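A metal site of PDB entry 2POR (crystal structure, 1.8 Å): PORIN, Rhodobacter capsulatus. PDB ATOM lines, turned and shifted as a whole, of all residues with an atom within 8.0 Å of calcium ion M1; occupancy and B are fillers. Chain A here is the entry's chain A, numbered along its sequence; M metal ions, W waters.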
ATOM      1  N   ASP A  85      -0.132  16.627  18.060  1.00  0.00           N
ATOM      2  CA  ASP A  85       0.629  16.640  19.297  1.00  0.00           C
ATOM      3  C   ASP A  85       2.109  16.784  19.048  1.00  0.00           C
ATOM      4  O   ASP A  85       2.551  16.748  17.908  1.00  0.00           O
ATOM      5  CB  ASP A  85       0.376  15.334  20.091  1.00  0.00           C
ATOM      6  CG  ASP A  85      -1.045  15.332  20.645  1.00  0.00           C
ATOM      7  OD1 ASP A  85      -1.552  16.366  21.072  1.00  0.00           O
ATOM      8  OD2 ASP A  85      -1.677  14.291  20.599  1.00  0.00           O
ATOM      9  N   LEU A  86       2.928  16.909  20.090  1.00  0.00           N
ATOM     10  CA  LEU A  86       4.364  17.041  19.969  1.00  0.00           C
ATOM     11  C   LEU A  86       4.902  15.621  19.879  1.00  0.00           C
ATOM     12  O   LEU A  86       4.144  14.643  19.994  1.00  0.00           O
ATOM     13  CB  LEU A  86       4.931  17.799  21.190  1.00  0.00           C
ATOM     14  CG  LEU A  86       4.407  19.214  21.458  1.00  0.00           C
ATOM     15  CD1 LEU A  86       5.260  19.743  22.598  1.00  0.00           C
ATOM     16  CD2 LEU A  86       4.533  20.163  20.256  1.00  0.00           C
ATOM     17  N   TYR A  87       6.208  15.484  19.650  1.00  0.00           N
ATOM     18  CA  TYR A  87       6.867  14.197  19.486  1.00  0.00           C
ATOM     19  C   TYR A  87       6.567  13.239  20.648  1.00  0.00           C
ATOM     20  O   TYR A  87       6.811  13.562  21.799  1.00  0.00           O
ATOM     21  CB  TYR A  87       8.397  14.408  19.373  1.00  0.00           C
ATOM     22  CG  TYR A  87       9.173  13.117  19.127  1.00  0.00           C
ATOM     23  CD1 TYR A  87       9.056  12.423  17.928  1.00  0.00           C
ATOM     24  CD2 TYR A  87       9.966  12.623  20.140  1.00  0.00           C
ATOM     25  CE1 TYR A  87       9.755  11.242  17.758  1.00  0.00           C
ATOM     26  CE2 TYR A  87      10.657  11.436  19.981  1.00  0.00           C
ATOM     27  CZ  TYR A  87      10.532  10.761  18.796  1.00  0.00           C
ATOM     28  OH  TYR A  87      11.177   9.560  18.680  1.00  0.00           O
ATOM     29  N   GLU A  88       6.106  12.024  20.376  1.00  0.00           N
ATOM     30  CA  GLU A  88       5.724  11.047  21.379  1.00  0.00           C
ATOM     31  C   GLU A  88       6.926  10.314  21.857  1.00  0.00           C
ATOM     32  O   GLU A  88       7.682   9.719  21.088  1.00  0.00           O
ATOM     33  CB  GLU A  88       4.690  10.112  20.765  1.00  0.00           C
ATOM     34  CG  GLU A  88       4.202   9.114  21.763  1.00  0.00           C
ATOM     35  CD  GLU A  88       3.049   8.235  21.281  1.00  0.00           C
ATOM     36  OE1 GLU A  88       2.009   8.725  20.873  1.00  0.00           O
ATOM     37  OE2 GLU A  88       3.187   7.034  21.357  1.00  0.00           O
ATOM     38  N   VAL A  89       7.101  10.369  23.155  1.00  0.00           N
ATOM     39  CA  VAL A  89       8.227   9.736  23.799  1.00  0.00           C
ATOM     40  C   VAL A  89       7.808   8.490  24.559  1.00  0.00           C
ATOM     41  O   VAL A  89       6.761   8.512  25.230  1.00  0.00           O
ATOM     42  CB  VAL A  89       8.877  10.784  24.741  1.00  0.00           C
ATOM     43  CG1 VAL A  89       9.939  10.108  25.614  1.00  0.00           C
ATOM     44  CG2 VAL A  89       9.474  11.919  23.913  1.00  0.00           C
ATOM     45  N   THR A  92       5.717   3.152  25.805  1.00  0.00           N
ATOM     46  CA  THR A  92       4.382   3.102  26.440  1.00  0.00           C
ATOM     47  C   THR A  92       3.668   4.457  26.301  1.00  0.00           C
ATOM     48  O   THR A  92       2.529   4.563  26.717  1.00  0.00           O
ATOM     49  CB  THR A  92       4.477   2.749  27.971  1.00  0.00           C
ATOM     50  OG1 THR A  92       5.254   3.777  28.570  1.00  0.00           O
ATOM     51  CG2 THR A  92       5.166   1.470  28.298  1.00  0.00           C
ATOM     52  N   ASP A  93       4.285   5.484  25.679  1.00  0.00           N
ATOM     53  CA  ASP A  93       3.826   6.874  25.564  1.00  0.00           C
ATOM     54  C   ASP A  93       3.819   7.432  26.976  1.00  0.00           C
ATOM     55  O   ASP A  93       2.812   7.401  27.705  1.00  0.00           O
ATOM     56  CB  ASP A  93       2.417   6.981  24.929  1.00  0.00           C
ATOM     57  CG  ASP A  93       1.904   8.396  24.716  1.00  0.00           C
ATOM     58  OD1 ASP A  93       2.587   9.404  24.905  1.00  0.00           O
ATOM     59  OD2 ASP A  93       0.747   8.549  24.340  1.00  0.00           O
ATOM     60  N   LEU A  94       5.000   7.900  27.413  1.00  0.00           N
ATOM     61  CA  LEU A  94       5.217   8.302  28.815  1.00  0.00           C
ATOM     62  C   LEU A  94       4.575   9.621  29.127  1.00  0.00           C
ATOM     63  O   LEU A  94       5.240  10.650  29.197  1.00  0.00           O
ATOM     64  CB  LEU A  94       6.696   8.406  29.135  1.00  0.00           C
ATOM     65  CG  LEU A  94       7.498   7.157  29.197  1.00  0.00           C
ATOM     66  CD1 LEU A  94       9.000   7.507  29.212  1.00  0.00           C
ATOM     67  CD2 LEU A  94       7.072   6.346  30.401  1.00  0.00           C
ATOM     68  N   ASP A  95       3.272   9.643  29.343  1.00  0.00           N
ATOM     69  CA  ASP A  95       2.550  10.858  29.637  1.00  0.00           C
ATOM     70  C   ASP A  95       2.383  11.126  31.131  1.00  0.00           C
ATOM     71  O   ASP A  95       1.749  12.080  31.563  1.00  0.00           O
ATOM     72  CB  ASP A  95       1.201  10.798  29.065  1.00  0.00           C
ATOM     73  CG  ASP A  95       1.151  10.967  27.574  1.00  0.00           C
ATOM     74  OD1 ASP A  95       1.980  11.649  26.987  1.00  0.00           O
ATOM     75  OD2 ASP A  95       0.260  10.424  26.953  1.00  0.00           O
ATOM     76  N   ASP A  96       2.978  10.272  31.932  1.00  0.00           N
ATOM     77  CA  ASP A  96       2.845  10.263  33.380  1.00  0.00           C
ATOM     78  C   ASP A  96       3.232  11.585  34.043  1.00  0.00           C
ATOM     79  O   ASP A  96       2.664  11.912  35.089  1.00  0.00           O
ATOM     80  CB  ASP A  96       3.721   9.126  33.920  1.00  0.00           C
ATOM     81  CG  ASP A  96       3.455   7.765  33.304  1.00  0.00           C
ATOM     82  OD1 ASP A  96       3.933   7.453  32.194  1.00  0.00           O
ATOM     83  OD2 ASP A  96       2.738   7.026  33.960  1.00  0.00           O
ATOM     84  N   GLY A  98       3.126  14.669  32.449  1.00  0.00           N
ATOM     85  CA  GLY A  98       2.596  15.761  31.627  1.00  0.00           C
ATOM     86  C   GLY A  98       2.335  15.315  30.169  1.00  0.00           C
ATOM     87  O   GLY A  98       1.299  15.644  29.567  1.00  0.00           O
ATOM     88  N   GLY A  99       3.347  14.637  29.650  1.00  0.00           N
ATOM     89  CA  GLY A  99       3.266  14.023  28.333  1.00  0.00           C
ATOM     90  C   GLY A  99       3.488  14.939  27.158  1.00  0.00           C
ATOM     91  O   GLY A  99       3.667  16.146  27.261  1.00  0.00           O
ATOM     92  N   ASN A 100       3.410  14.354  25.986  1.00  0.00           N
ATOM     93  CA  ASN A 100       3.720  15.062  24.730  1.00  0.00           C
ATOM     94  C   ASN A 100       2.503  15.729  24.158  1.00  0.00           C
ATOM     95  O   ASN A 100       2.588  16.505  23.215  1.00  0.00           O
ATOM     96  CB  ASN A 100       4.286  14.038  23.737  1.00  0.00           C
ATOM     97  CG  ASN A 100       3.261  12.979  23.352  1.00  0.00           C
ATOM     98  OD1 ASN A 100       2.744  12.222  24.170  1.00  0.00           O
ATOM     99  ND2 ASN A 100       2.889  12.911  22.084  1.00  0.00           N
ATOM    100  N   ASP A 101       1.306  15.431  24.630  1.00  0.00           N
ATOM    101  CA  ASP A 101       0.084  15.937  24.044  1.00  0.00           C
ATOM    102  C   ASP A 101      -0.067  17.406  24.206  1.00  0.00           C
ATOM    103  O   ASP A 101       0.283  17.946  25.246  1.00  0.00           O
ATOM    104  CB  ASP A 101      -1.121  15.252  24.691  1.00  0.00           C
ATOM    105  CG  ASP A 101      -1.086  13.723  24.650  1.00  0.00           C
ATOM    106  OD1 ASP A 101      -0.058  13.020  24.767  1.00  0.00           O
ATOM    107  OD2 ASP A 101      -2.176  13.221  24.466  1.00  0.00           O
ATOM    108  N   ILE A 102      -0.541  18.112  23.211  1.00  0.00           N
ATOM    109  CA  ILE A 102      -0.735  19.527  23.352  1.00  0.00           C
ATOM    110  C   ILE A 102      -2.043  19.699  24.152  1.00  0.00           C
ATOM    111  O   ILE A 102      -2.992  18.926  23.930  1.00  0.00           O
ATOM    112  CB  ILE A 102      -0.764  20.157  21.908  1.00  0.00           C
ATOM    113  CG1 ILE A 102       0.663  20.192  21.337  1.00  0.00           C
ATOM    114  CG2 ILE A 102      -1.365  21.571  21.927  1.00  0.00           C
ATOM    115  CD1 ILE A 102       0.708  20.766  19.876  1.00  0.00           C
ATOM    116  N   TYR A 248      10.675  17.106  23.548  1.00  0.00           N
ATOM    117  CA  TYR A 248       9.756  18.221  23.551  1.00  0.00           C
ATOM    118  C   TYR A 248       9.884  18.937  24.897  1.00  0.00           C
ATOM    119  O   TYR A 248      10.415  18.325  25.863  1.00  0.00           O
ATOM    120  CB  TYR A 248       8.300  17.730  23.371  1.00  0.00           C
ATOM    121  CG  TYR A 248       7.791  16.828  24.499  1.00  0.00           C
ATOM    122  CD1 TYR A 248       7.246  17.429  25.631  1.00  0.00           C
ATOM    123  CD2 TYR A 248       7.933  15.446  24.485  1.00  0.00           C
ATOM    124  CE1 TYR A 248       6.851  16.653  26.717  1.00  0.00           C
ATOM    125  CE2 TYR A 248       7.538  14.670  25.571  1.00  0.00           C
ATOM    126  CZ  TYR A 248       6.989  15.286  26.708  1.00  0.00           C
ATOM    127  OH  TYR A 248       6.578  14.573  27.838  1.00  0.00           O
HETATM  128 CA    CA M   1       0.873  10.969  24.701  1.00  0.00          CA
HETATM  129 CA    CA M   2      -5.527  15.191  22.663  1.00  0.00          CA
HETATM  130  O   HOH W   1      -1.313  10.605  24.323  1.00  0.00           O
HETATM  131  O   HOH W   2       0.899  10.910  22.313  1.00  0.00           O
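The backbone carbonyl oxygen (O) of Leu 86 lies within hydrogen-bond range of the side-chain amide nitrogen (ND2) of Asn 100, at 3.0 Å.
Of the 16 residues printed, 4 come within 4 Å of calcium ion M1.
The nearest printed residue that does not touch calcium ion M1 is Glu 88 (4.6 Å).
Water W1 is bound to calcium ion M1.
Calcium ion M1 is bound by OD1 of Asp 101 (2.3 Å).
Calcium ion M1 is bound by the side-chain amide oxygen (OD1) of Asn 100 (2.3 Å).
OD1 of Asp 93 is bound to calcium ion M1 (2.3 Å).
Calcium ion M1 is bound by water W2 (2.4 Å).
OD2 of Asp 95 binds calcium ion M1, at 2.4 Å.
OD2 of Asp 93 is bound to calcium ion M1 (2.5 Å).
OD1 of Asp 95 binds calcium ion M1 (2.6 Å).
Calcium ion M1 has eight donor atoms within binding distance.
Water W2 bridges the side-chain amide nitrogen (ND2) of Asn 100 (2.8 Å) and the side-chain carboxylate (OE1) of Glu 88 (2.8 Å).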
